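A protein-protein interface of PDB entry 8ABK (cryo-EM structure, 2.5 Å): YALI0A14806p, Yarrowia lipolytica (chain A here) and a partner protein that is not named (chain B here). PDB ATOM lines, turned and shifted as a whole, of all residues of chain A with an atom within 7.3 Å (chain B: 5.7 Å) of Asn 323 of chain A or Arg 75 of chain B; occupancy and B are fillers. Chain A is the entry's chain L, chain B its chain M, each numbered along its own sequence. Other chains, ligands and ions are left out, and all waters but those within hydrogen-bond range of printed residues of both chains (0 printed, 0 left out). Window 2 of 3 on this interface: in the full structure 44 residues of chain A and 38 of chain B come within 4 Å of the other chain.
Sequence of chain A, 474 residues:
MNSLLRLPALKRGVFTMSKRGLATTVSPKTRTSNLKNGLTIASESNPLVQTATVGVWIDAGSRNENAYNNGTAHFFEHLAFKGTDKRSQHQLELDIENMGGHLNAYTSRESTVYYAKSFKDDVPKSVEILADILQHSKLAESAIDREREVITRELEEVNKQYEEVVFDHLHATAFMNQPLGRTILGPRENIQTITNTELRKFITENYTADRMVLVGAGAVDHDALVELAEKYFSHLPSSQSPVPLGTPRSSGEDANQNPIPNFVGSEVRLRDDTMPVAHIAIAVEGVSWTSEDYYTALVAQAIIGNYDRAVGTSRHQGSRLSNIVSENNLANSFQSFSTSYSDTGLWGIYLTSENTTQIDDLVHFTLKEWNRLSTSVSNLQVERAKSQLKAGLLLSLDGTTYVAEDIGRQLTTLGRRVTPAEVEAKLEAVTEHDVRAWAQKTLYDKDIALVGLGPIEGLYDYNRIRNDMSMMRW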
ATOM      1  N   TYR A 307     -25.840  -3.484 -17.030  1.00  0.00           N
ATOM      2  CA  TYR A 307     -27.183  -4.003 -17.110  1.00  0.00           C
ATOM      3  C   TYR A 307     -27.645  -3.902 -18.553  1.00  0.00           C
ATOM      4  O   TYR A 307     -27.345  -2.912 -19.206  1.00  0.00           O
ATOM      5  CB  TYR A 307     -28.104  -3.103 -16.298  1.00  0.00           C
ATOM      6  CG  TYR A 307     -29.550  -3.398 -16.557  1.00  0.00           C
ATOM      7  CD1 TYR A 307     -30.140  -4.515 -15.979  1.00  0.00           C
ATOM      8  CD2 TYR A 307     -30.303  -2.589 -17.403  1.00  0.00           C
ATOM      9  CE1 TYR A 307     -31.478  -4.795 -16.203  1.00  0.00           C
ATOM     10  CE2 TYR A 307     -31.639  -2.870 -17.652  1.00  0.00           C
ATOM     11  CZ  TYR A 307     -32.217  -3.976 -17.051  1.00  0.00           C
ATOM     12  OH  TYR A 307     -33.529  -4.243 -17.281  1.00  0.00           O
ATOM     13  N   THR A 313     -30.295 -12.782 -17.825  1.00  0.00           N
ATOM     14  CA  THR A 313     -29.845 -12.856 -16.446  1.00  0.00           C
ATOM     15  C   THR A 313     -29.887 -11.489 -15.759  1.00  0.00           C
ATOM     16  O   THR A 313     -29.783 -11.434 -14.536  1.00  0.00           O
ATOM     17  CB  THR A 313     -28.424 -13.418 -16.338  1.00  0.00           C
ATOM     18  OG1 THR A 313     -27.630 -12.577 -17.173  1.00  0.00           O
ATOM     19  CG2 THR A 313     -28.299 -14.869 -16.753  1.00  0.00           C
ATOM     20  N   SER A 314     -30.024 -10.394 -16.523  1.00  0.00           N
ATOM     21  CA  SER A 314     -29.734  -9.078 -15.968  1.00  0.00           C
ATOM     22  C   SER A 314     -30.778  -8.656 -14.934  1.00  0.00           C
ATOM     23  O   SER A 314     -30.484  -7.879 -14.038  1.00  0.00           O
ATOM     24  CB  SER A 314     -29.573  -8.050 -17.053  1.00  0.00           C
ATOM     25  OG  SER A 314     -30.818  -7.869 -17.704  1.00  0.00           O
ATOM     26  N   ARG A 315     -31.991  -9.195 -15.018  1.00  0.00           N
ATOM     27  CA  ARG A 315     -32.979  -8.861 -14.010  1.00  0.00           C
ATOM     28  C   ARG A 315     -32.641  -9.481 -12.650  1.00  0.00           C
ATOM     29  O   ARG A 315     -33.248  -9.123 -11.651  1.00  0.00           O
ATOM     30  CB  ARG A 315     -34.358  -9.299 -14.486  1.00  0.00           C
ATOM     31  CG  ARG A 315     -34.612 -10.778 -14.267  1.00  0.00           C
ATOM     32  CD  ARG A 315     -36.071 -11.134 -14.450  1.00  0.00           C
ATOM     33  NE  ARG A 315     -36.432 -10.972 -15.851  1.00  0.00           N
ATOM     34  CZ  ARG A 315     -37.363 -10.144 -16.318  1.00  0.00           C
ATOM     35  NH1 ARG A 315     -38.085  -9.398 -15.496  1.00  0.00           N
ATOM     36  NH2 ARG A 315     -37.589 -10.089 -17.619  1.00  0.00           N
ATOM     37  N   HIS A 316     -31.664 -10.383 -12.593  1.00  0.00           N
ATOM     38  CA  HIS A 316     -31.395 -11.073 -11.346  1.00  0.00           C
ATOM     39  C   HIS A 316     -30.092 -10.632 -10.699  1.00  0.00           C
ATOM     40  O   HIS A 316     -29.734 -11.170  -9.656  1.00  0.00           O
ATOM     41  CB  HIS A 316     -31.355 -12.571 -11.603  1.00  0.00           C
ATOM     42  CG  HIS A 316     -32.676 -13.113 -12.005  1.00  0.00           C
ATOM     43  ND1 HIS A 316     -33.811 -12.897 -11.250  1.00  0.00           N
ATOM     44  CD2 HIS A 316     -33.056 -13.834 -13.081  1.00  0.00           C
ATOM     45  CE1 HIS A 316     -34.834 -13.489 -11.828  1.00  0.00           C
ATOM     46  NE2 HIS A 316     -34.396 -14.073 -12.956  1.00  0.00           N
ATOM     47  N   GLN A 317     -29.384  -9.688 -11.320  1.00  0.00           N
ATOM     48  CA  GLN A 317     -28.074  -9.260 -10.848  1.00  0.00           C
ATOM     49  C   GLN A 317     -28.164  -8.655  -9.452  1.00  0.00           C
ATOM     50  O   GLN A 317     -29.170  -8.049  -9.088  1.00  0.00           O
ATOM     51  CB  GLN A 317     -27.508  -8.202 -11.789  1.00  0.00           C
ATOM     52  CG  GLN A 317     -27.162  -8.764 -13.150  1.00  0.00           C
ATOM     53  CD  GLN A 317     -26.511  -7.748 -14.050  1.00  0.00           C
ATOM     54  OE1 GLN A 317     -25.456  -8.008 -14.621  1.00  0.00           O
ATOM     55  NE2 GLN A 317     -27.137  -6.589 -14.202  1.00  0.00           N
ATOM     56  N   GLY A 318     -27.066  -8.776  -8.700  1.00  0.00           N
ATOM     57  CA  GLY A 318     -26.997  -8.335  -7.313  1.00  0.00           C
ATOM     58  C   GLY A 318     -26.895  -6.819  -7.135  1.00  0.00           C
ATOM     59  O   GLY A 318     -27.290  -6.298  -6.089  1.00  0.00           O
ATOM     60  N   SER A 319     -26.362  -6.124  -8.149  1.00  0.00           N
ATOM     61  CA  SER A 319     -26.171  -4.680  -8.141  1.00  0.00           C
ATOM     62  C   SER A 319     -27.476  -3.966  -7.799  1.00  0.00           C
ATOM     63  O   SER A 319     -28.490  -4.212  -8.438  1.00  0.00           O
ATOM     64  CB  SER A 319     -25.646  -4.223  -9.476  1.00  0.00           C
ATOM     65  OG  SER A 319     -25.806  -2.818  -9.648  1.00  0.00           O
ATOM     66  N   ARG A 320     -27.428  -3.048  -6.826  1.00  0.00           N
ATOM     67  CA  ARG A 320     -28.607  -2.295  -6.431  1.00  0.00           C
ATOM     68  C   ARG A 320     -29.180  -1.486  -7.595  1.00  0.00           C
ATOM     69  O   ARG A 320     -30.401  -1.440  -7.778  1.00  0.00           O
ATOM     70  CB  ARG A 320     -28.313  -1.420  -5.210  1.00  0.00           C
ATOM     71  CG  ARG A 320     -29.451  -0.474  -4.855  1.00  0.00           C
ATOM     72  CD  ARG A 320     -30.693  -1.240  -4.435  1.00  0.00           C
ATOM     73  NE  ARG A 320     -31.787  -0.387  -3.996  1.00  0.00           N
ATOM     74  CZ  ARG A 320     -33.059  -0.770  -3.876  1.00  0.00           C
ATOM     75  NH1 ARG A 320     -33.418  -2.010  -4.170  1.00  0.00           N
ATOM     76  NH2 ARG A 320     -33.968   0.097  -3.467  1.00  0.00           N
ATOM     77  N   LEU A 321     -28.297  -0.816  -8.351  1.00  0.00           N
ATOM     78  CA  LEU A 321     -28.747   0.027  -9.448  1.00  0.00           C
ATOM     79  C   LEU A 321     -29.452  -0.835 -10.484  1.00  0.00           C
ATOM     80  O   LEU A 321     -30.488  -0.437 -11.014  1.00  0.00           O
ATOM     81  CB  LEU A 321     -27.597   0.813 -10.087  1.00  0.00           C
ATOM     82  CG  LEU A 321     -28.044   1.734 -11.231  1.00  0.00           C
ATOM     83  CD1 LEU A 321     -29.061   2.773 -10.763  1.00  0.00           C
ATOM     84  CD2 LEU A 321     -26.873   2.395 -11.940  1.00  0.00           C
ATOM     85  N   SER A 322     -28.888  -2.021 -10.738  1.00  0.00           N
ATOM     86  CA  SER A 322     -29.502  -2.965 -11.651  1.00  0.00           C
ATOM     87  C   SER A 322     -30.936  -3.267 -11.222  1.00  0.00           C
ATOM     88  O   SER A 322     -31.836  -3.237 -12.053  1.00  0.00           O
ATOM     89  CB  SER A 322     -28.691  -4.214 -11.729  1.00  0.00           C
ATOM     90  OG  SER A 322     -29.240  -5.101 -12.684  1.00  0.00           O
ATOM     91  N   ASN A 323     -31.138  -3.550  -9.932  1.00  0.00           N
ATOM     92  CA  ASN A 323     -32.457  -3.868  -9.413  1.00  0.00           C
ATOM     93  C   ASN A 323     -33.411  -2.696  -9.607  1.00  0.00           C
ATOM     94  O   ASN A 323     -34.515  -2.906 -10.091  1.00  0.00           O
ATOM     95  CB  ASN A 323     -32.402  -4.332  -7.961  1.00  0.00           C
ATOM     96  CG  ASN A 323     -31.813  -5.720  -7.851  1.00  0.00           C
ATOM     97  OD1 ASN A 323     -32.481  -6.701  -8.167  1.00  0.00           O
ATOM     98  ND2 ASN A 323     -30.559  -5.820  -7.439  1.00  0.00           N
ATOM     99  N   ILE A 324     -32.976  -1.472  -9.280  1.00  0.00           N
ATOM    100  CA  ILE A 324     -33.853  -0.311  -9.389  1.00  0.00           C
ATOM    101  C   ILE A 324     -34.274  -0.124 -10.845  1.00  0.00           C
ATOM    102  O   ILE A 324     -35.436   0.148 -11.135  1.00  0.00           O
ATOM    103  CB  ILE A 324     -33.177   0.967  -8.848  1.00  0.00           C
ATOM    104  CG1 ILE A 324     -32.940   0.902  -7.337  1.00  0.00           C
ATOM    105  CG2 ILE A 324     -33.960   2.220  -9.237  1.00  0.00           C
ATOM    106  CD1 ILE A 324     -31.786   1.759  -6.849  1.00  0.00           C
ATOM    107  N   VAL A 325     -33.295  -0.206 -11.738  1.00  0.00           N
ATOM    108  CA  VAL A 325     -33.504   0.083 -13.139  1.00  0.00           C
ATOM    109  C   VAL A 325     -34.394  -0.980 -13.773  1.00  0.00           C
ATOM    110  O   VAL A 325     -35.303  -0.636 -14.525  1.00  0.00           O
ATOM    111  CB  VAL A 325     -32.164   0.265 -13.865  1.00  0.00           C
ATOM    112  CG1 VAL A 325     -32.332   0.173 -15.370  1.00  0.00           C
ATOM    113  CG2 VAL A 325     -31.553   1.598 -13.473  1.00  0.00           C
ATOM    114  N   SER A 326     -34.156  -2.251 -13.450  1.00  0.00           N
ATOM    115  CA  SER A 326     -34.967  -3.291 -14.062  1.00  0.00           C
ATOM    116  C   SER A 326     -36.393  -3.273 -13.520  1.00  0.00           C
ATOM    117  O   SER A 326     -37.314  -3.352 -14.317  1.00  0.00           O
ATOM    118  CB  SER A 326     -34.343  -4.647 -13.992  1.00  0.00           C
ATOM    119  OG  SER A 326     -34.141  -5.016 -12.645  1.00  0.00           O
ATOM    120  N   GLU A 327     -36.584  -3.103 -12.198  1.00  0.00           N
ATOM    121  CA  GLU A 327     -37.932  -3.099 -11.624  1.00  0.00           C
ATOM    122  C   GLU A 327     -38.791  -1.956 -12.172  1.00  0.00           C
ATOM    123  O   GLU A 327     -40.008  -2.074 -12.312  1.00  0.00           O
ATOM    124  CB  GLU A 327     -37.909  -3.009 -10.097  1.00  0.00           C
ATOM    125  CG  GLU A 327     -37.399  -4.270  -9.426  1.00  0.00           C
ATOM    126  CD  GLU A 327     -37.159  -4.165  -7.927  1.00  0.00           C
ATOM    127  OE1 GLU A 327     -36.281  -3.377  -7.509  1.00  0.00           O
ATOM    128  OE2 GLU A 327     -37.859  -4.874  -7.174  1.00  0.00           O
ATOM    129  N   ASN A 328     -38.153  -0.835 -12.475  1.00  0.00           N
ATOM    130  CA  ASN A 328     -38.887   0.363 -12.809  1.00  0.00           C
ATOM    131  C   ASN A 328     -38.849   0.639 -14.302  1.00  0.00           C
ATOM    132  O   ASN A 328     -39.355   1.674 -14.732  1.00  0.00           O
ATOM    133  CB  ASN A 328     -38.331   1.510 -11.981  1.00  0.00           C
ATOM    134  CG  ASN A 328     -38.712   1.308 -10.536  1.00  0.00           C
ATOM    135  OD1 ASN A 328     -39.887   1.401 -10.190  1.00  0.00           O
ATOM    136  ND2 ASN A 328     -37.751   0.963  -9.700  1.00  0.00           N
ATOM    137  N   ASN A 329     -38.214  -0.243 -15.083  1.00  0.00           N
ATOM    138  CA  ASN A 329     -38.043  -0.021 -16.516  1.00  0.00           C
ATOM    139  C   ASN A 329     -37.411   1.337 -16.816  1.00  0.00           C
ATOM    140  O   ASN A 329     -37.848   2.069 -17.695  1.00  0.00           O
ATOM    141  CB  ASN A 329     -39.341  -0.265 -17.284  1.00  0.00           C
ATOM    142  CG  ASN A 329     -39.896  -1.621 -16.927  1.00  0.00           C
ATOM    143  OD1 ASN A 329     -40.924  -1.721 -16.264  1.00  0.00           O
ATOM    144  ND2 ASN A 329     -39.177  -2.671 -17.294  1.00  0.00           N
ATOM    145  N   PHE A 334     -27.219  -0.001 -19.070  1.00  0.00           N
ATOM    146  CA  PHE A 334     -26.187   0.874 -18.559  1.00  0.00           C
ATOM    147  C   PHE A 334     -24.896   0.087 -18.477  1.00  0.00           C
ATOM    148  O   PHE A 334     -24.932  -1.125 -18.306  1.00  0.00           O
ATOM    149  CB  PHE A 334     -26.593   1.524 -17.239  1.00  0.00           C
ATOM    150  CG  PHE A 334     -26.762   0.627 -16.043  1.00  0.00           C
ATOM    151  CD1 PHE A 334     -25.655   0.081 -15.396  1.00  0.00           C
ATOM    152  CD2 PHE A 334     -28.033   0.395 -15.524  1.00  0.00           C
ATOM    153  CE1 PHE A 334     -25.819  -0.692 -14.257  1.00  0.00           C
ATOM    154  CE2 PHE A 334     -28.190  -0.366 -14.375  1.00  0.00           C
ATOM    155  CZ  PHE A 334     -27.084  -0.914 -13.744  1.00  0.00           C
ATOM    156  N   ARG A 384     -18.162  -9.013  -2.723  1.00  0.00           N
ATOM    157  CA  ARG A 384     -18.871  -9.577  -3.854  1.00  0.00           C
ATOM    158  C   ARG A 384     -18.227  -9.124  -5.168  1.00  0.00           C
ATOM    159  O   ARG A 384     -18.116  -9.916  -6.099  1.00  0.00           O
ATOM    160  CB  ARG A 384     -20.348  -9.206  -3.786  1.00  0.00           C
ATOM    161  CG  ARG A 384     -21.204 -10.128  -2.929  1.00  0.00           C
ATOM    162  CD  ARG A 384     -22.686  -9.856  -3.137  1.00  0.00           C
ATOM    163  NE  ARG A 384     -23.131  -8.495  -2.848  1.00  0.00           N
ATOM    164  CZ  ARG A 384     -23.757  -7.662  -3.684  1.00  0.00           C
ATOM    165  NH1 ARG A 384     -24.068  -6.446  -3.267  1.00  0.00           N
ATOM    166  NH2 ARG A 384     -24.079  -8.025  -4.917  1.00  0.00           N
ATOM    167  N   ALA B  70     -33.838 -19.267 -10.654  1.00  0.00           N
ATOM    168  CA  ALA B  70     -33.084 -18.444 -11.590  1.00  0.00           C
ATOM    169  C   ALA B  70     -32.326 -17.345 -10.843  1.00  0.00           C
ATOM    170  O   ALA B  70     -31.162 -17.064 -11.137  1.00  0.00           O
ATOM    171  CB  ALA B  70     -34.007 -17.881 -12.645  1.00  0.00           C
ATOM    172  N   LEU B  71     -32.987 -16.747  -9.853  1.00  0.00           N
ATOM    173  CA  LEU B  71     -32.394 -15.663  -9.099  1.00  0.00           C
ATOM    174  C   LEU B  71     -31.201 -16.201  -8.322  1.00  0.00           C
ATOM    175  O   LEU B  71     -30.124 -15.623  -8.365  1.00  0.00           O
ATOM    176  CB  LEU B  71     -33.455 -15.075  -8.170  1.00  0.00           C
ATOM    177  CG  LEU B  71     -32.931 -14.282  -6.974  1.00  0.00           C
ATOM    178  CD1 LEU B  71     -32.311 -12.958  -7.406  1.00  0.00           C
ATOM    179  CD2 LEU B  71     -34.060 -14.021  -5.989  1.00  0.00           C
ATOM    180  N   ARG B  72     -31.386 -17.320  -7.633  1.00  0.00           N
ATOM    181  CA  ARG B  72     -30.258 -17.800  -6.863  1.00  0.00           C
ATOM    182  C   ARG B  72     -29.091 -18.204  -7.766  1.00  0.00           C
ATOM    183  O   ARG B  72     -27.938 -18.039  -7.384  1.00  0.00           O
ATOM    184  CB  ARG B  72     -30.652 -19.002  -6.025  1.00  0.00           C
ATOM    185  CG  ARG B  72     -29.443 -19.505  -5.261  1.00  0.00           C
ATOM    186  CD  ARG B  72     -29.714 -20.204  -3.954  1.00  0.00           C
ATOM    187  NE  ARG B  72     -30.666 -19.517  -3.095  1.00  0.00           N
ATOM    188  CZ  ARG B  72     -30.397 -19.042  -1.884  1.00  0.00           C
ATOM    189  NH1 ARG B  72     -29.183 -19.156  -1.370  1.00  0.00           N
ATOM    190  NH2 ARG B  72     -31.352 -18.445  -1.194  1.00  0.00           N
ATOM    191  N   PHE B  73     -29.392 -18.776  -8.933  1.00  0.00           N
ATOM    192  CA  PHE B  73     -28.349 -19.143  -9.873  1.00  0.00           C
ATOM    193  C   PHE B  73     -27.537 -17.922 -10.303  1.00  0.00           C
ATOM    194  O   PHE B  73     -26.313 -17.952 -10.244  1.00  0.00           O
ATOM    195  CB  PHE B  73     -28.925 -19.853 -11.097  1.00  0.00           C
ATOM    196  CG  PHE B  73     -27.855 -20.176 -12.104  1.00  0.00           C
ATOM    197  CD1 PHE B  73     -26.871 -21.112 -11.809  1.00  0.00           C
ATOM    198  CD2 PHE B  73     -27.788 -19.504 -13.317  1.00  0.00           C
ATOM    199  CE1 PHE B  73     -25.868 -21.404 -12.725  1.00  0.00           C
ATOM    200  CE2 PHE B  73     -26.781 -19.789 -14.235  1.00  0.00           C
ATOM    201  CZ  PHE B  73     -25.823 -20.739 -13.935  1.00  0.00           C
ATOM    202  N   VAL B  74     -28.214 -16.851 -10.729  1.00  0.00           N
ATOM    203  CA  VAL B  74     -27.514 -15.664 -11.186  1.00  0.00           C
ATOM    204  C   VAL B  74     -26.691 -15.059 -10.052  1.00  0.00           C
ATOM    205  O   VAL B  74     -25.584 -14.611 -10.302  1.00  0.00           O
ATOM    206  CB  VAL B  74     -28.482 -14.630 -11.781  1.00  0.00           C
ATOM    207  CG1 VAL B  74     -27.819 -13.277 -12.003  1.00  0.00           C
ATOM    208  CG2 VAL B  74     -29.140 -15.142 -13.049  1.00  0.00           C
ATOM    209  N   ARG B  75     -27.214 -15.023  -8.822  1.00  0.00           N
ATOM    210  CA  ARG B  75     -26.436 -14.418  -7.748  1.00  0.00           C
ATOM    211  C   ARG B  75     -25.206 -15.265  -7.420  1.00  0.00           C
ATOM    212  O   ARG B  75     -24.173 -14.729  -7.031  1.00  0.00           O
ATOM    213  CB  ARG B  75     -27.246 -14.200  -6.466  1.00  0.00           C
ATOM    214  CG  ARG B  75     -28.420 -13.244  -6.592  1.00  0.00           C
ATOM    215  CD  ARG B  75     -28.021 -11.845  -7.015  1.00  0.00           C
ATOM    216  NE  ARG B  75     -29.205 -11.008  -7.035  1.00  0.00           N
ATOM    217  CZ  ARG B  75     -29.660 -10.313  -6.000  1.00  0.00           C
ATOM    218  NH1 ARG B  75     -29.017 -10.340  -4.844  1.00  0.00           N
ATOM    219  NH2 ARG B  75     -30.757  -9.589  -6.129  1.00  0.00           N
ATOM    220  N   GLU B  76     -25.290 -16.582  -7.605  1.00  0.00           N
ATOM    221  CA  GLU B  76     -24.145 -17.400  -7.247  1.00  0.00           C
ATOM    222  C   GLU B  76     -23.136 -17.421  -8.381  1.00  0.00           C
ATOM    223  O   GLU B  76     -21.938 -17.513  -8.130  1.00  0.00           O
ATOM    224  CB  GLU B  76     -24.544 -18.832  -6.937  1.00  0.00           C
ATOM    225  CG  GLU B  76     -25.167 -18.964  -5.575  1.00  0.00           C
ATOM    226  CD  GLU B  76     -25.803 -20.315  -5.299  1.00  0.00           C
ATOM    227  OE1 GLU B  76     -26.132 -20.579  -4.124  1.00  0.00           O
ATOM    228  OE2 GLU B  76     -25.958 -21.112  -6.249  1.00  0.00           O
ATOM    229  N   LEU B  77     -23.633 -17.348  -9.619  1.00  0.00           N
ATOM    230  CA  LEU B  77     -22.768 -17.246 -10.780  1.00  0.00           C
ATOM    231  C   LEU B  77     -21.905 -15.980 -10.699  1.00  0.00           C
ATOM    232  O   LEU B  77     -20.756 -15.992 -11.135  1.00  0.00           O
ATOM    233  CB  LEU B  77     -23.660 -17.267 -12.024  1.00  0.00           C
ATOM    234  CG  LEU B  77     -22.985 -17.028 -13.372  1.00  0.00           C
ATOM    235  CD1 LEU B  77     -22.459 -18.332 -13.950  1.00  0.00           C
ATOM    236  CD2 LEU B  77     -23.974 -16.405 -14.346  1.00  0.00           C
ATOM    237  N   GLU B  78     -22.446 -14.893 -10.126  1.00  0.00           N
ATOM    238  CA  GLU B  78     -21.702 -13.651  -9.946  1.00  0.00           C
ATOM    239  C   GLU B  78     -20.627 -13.810  -8.878  1.00  0.00           C
ATOM    240  O   GLU B  78     -19.581 -13.178  -8.999  1.00  0.00           O
ATOM    241  CB  GLU B  78     -22.595 -12.466  -9.574  1.00  0.00           C
ATOM    242  CG  GLU B  78     -23.560 -12.045 -10.672  1.00  0.00           C
ATOM    243  CD  GLU B  78     -24.622 -11.028 -10.266  1.00  0.00           C
ATOM    244  OE1 GLU B  78     -24.726  -9.964 -10.927  1.00  0.00           O
ATOM    245  OE2 GLU B  78     -25.370 -11.318  -9.308  1.00  0.00           O
ATOM    246  N   LEU B  79     -20.846 -14.679  -7.883  1.00  0.00           N
ATOM    247  CA  LEU B  79     -19.819 -14.920  -6.872  1.00  0.00           C
ATOM    248  C   LEU B  79     -18.657 -15.742  -7.414  1.00  0.00           C
ATOM    249  O   LEU B  79     -17.571 -15.732  -6.832  1.00  0.00           O
ATOM    250  CB  LEU B  79     -20.402 -15.664  -5.672  1.00  0.00           C
ATOM    251  CG  LEU B  79     -21.495 -14.929  -4.918  1.00  0.00           C
ATOM    252  CD1 LEU B  79     -22.016 -15.782  -3.776  1.00  0.00           C
ATOM    253  CD2 LEU B  79     -21.020 -13.577  -4.413  1.00  0.00           C
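The guanidinium group (NE) of Arg 75 of chain B lies within hydrogen-bond range of the backbone carbonyl oxygen (O) of His 316 of chain A (2.7 Å).
N of Gly 318 of chain A sits at hydrogen-bond distance from OE2 of Glu 78 of chain B (3.1 Å).
The side-chain amide nitrogen of Gln 317 of chain A sits at hydrogen-bond distance from the side-chain hydroxyl of Ser 322 of chain A (3.0 Å).
The side-chain amide nitrogen (ND2) of Asn 323 of chain A sits at hydrogen-bond distance from the backbone carbonyl oxygen (O) of Gln 317 of chain A (3.1 Å).
The side-chain amide nitrogen of Asn 323 of chain A lies within hydrogen-bond range of the backbone carbonyl oxygen of Ser 319 of chain A, at 2.8 Å.
OG of Ser 326 of chain A sits at hydrogen-bond distance from O of Asn 323 of chain A (3.3 Å).
Among the printed residues, pairs that only touch across the chains: Gln 317 of chain A with Glu 78 of chain B, Gly 318 of chain A with Arg 75 of chain B, Gln 317 of chain A with Arg 75 of chain B, His 316 of chain A with Val 74 of chain B, Thr 313 of chain A with Val 74 of chain B, Arg 384 of chain A with Leu 79 of chain B, His 316 of chain A with Leu 71 of chain B, His 316 of chain A with Ala 70 of chain B, Asn 323 of chain A with Arg 75 of chain B and Gln 317 of chain A with Val 74 of chain B.
Of the printed residues of chain B, Thr 313 of chain A touches Val 74 (3.7 Å).
Asn 323 of chain A touches just one residue of chain B: Arg 75 (3.9 Å).
Ile 324 of chain A touches none of the printed residues of chain B.
Val 325 of chain A touches none of the printed residues of chain B.
Of the printed residues of chain B, Arg 384 of chain A touches Leu 79 (3.8 Å).
Printed residues of chain A within 4 Å of Leu 71 of chain B: His 316 (3.8 Å).
Of the printed residues of chain A, Glu 78 of chain B touches Gln 317 (3.4 Å) and Gly 318 (3.1 Å).
The nearest residue of chain A that does not touch Arg 75 of chain B is Arg 384 of chain A (5.5 Å).
The nearest printed residue of chain B that does not touch Gly 318 of chain A is Val 74 of chain B (5.6 Å).
Of the 10 printed residues of chain B, 6 touch a printed residue of chain A.
Hydrophobic or aromatic side chains of chain B that line the printed part of chain A: Ala 70, Leu 71, Val 74 and Leu 79.
Of the 20 printed residues of chain A, 6 touch a printed residue of chain B.
Hydrophobic or aromatic side chains of chain A that line the printed part of chain B: His 316.
Among the printed residues, no Asp or Glu carboxylate lies within 4 Å of a Lys or Arg side-chain nitrogen of the other chain.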
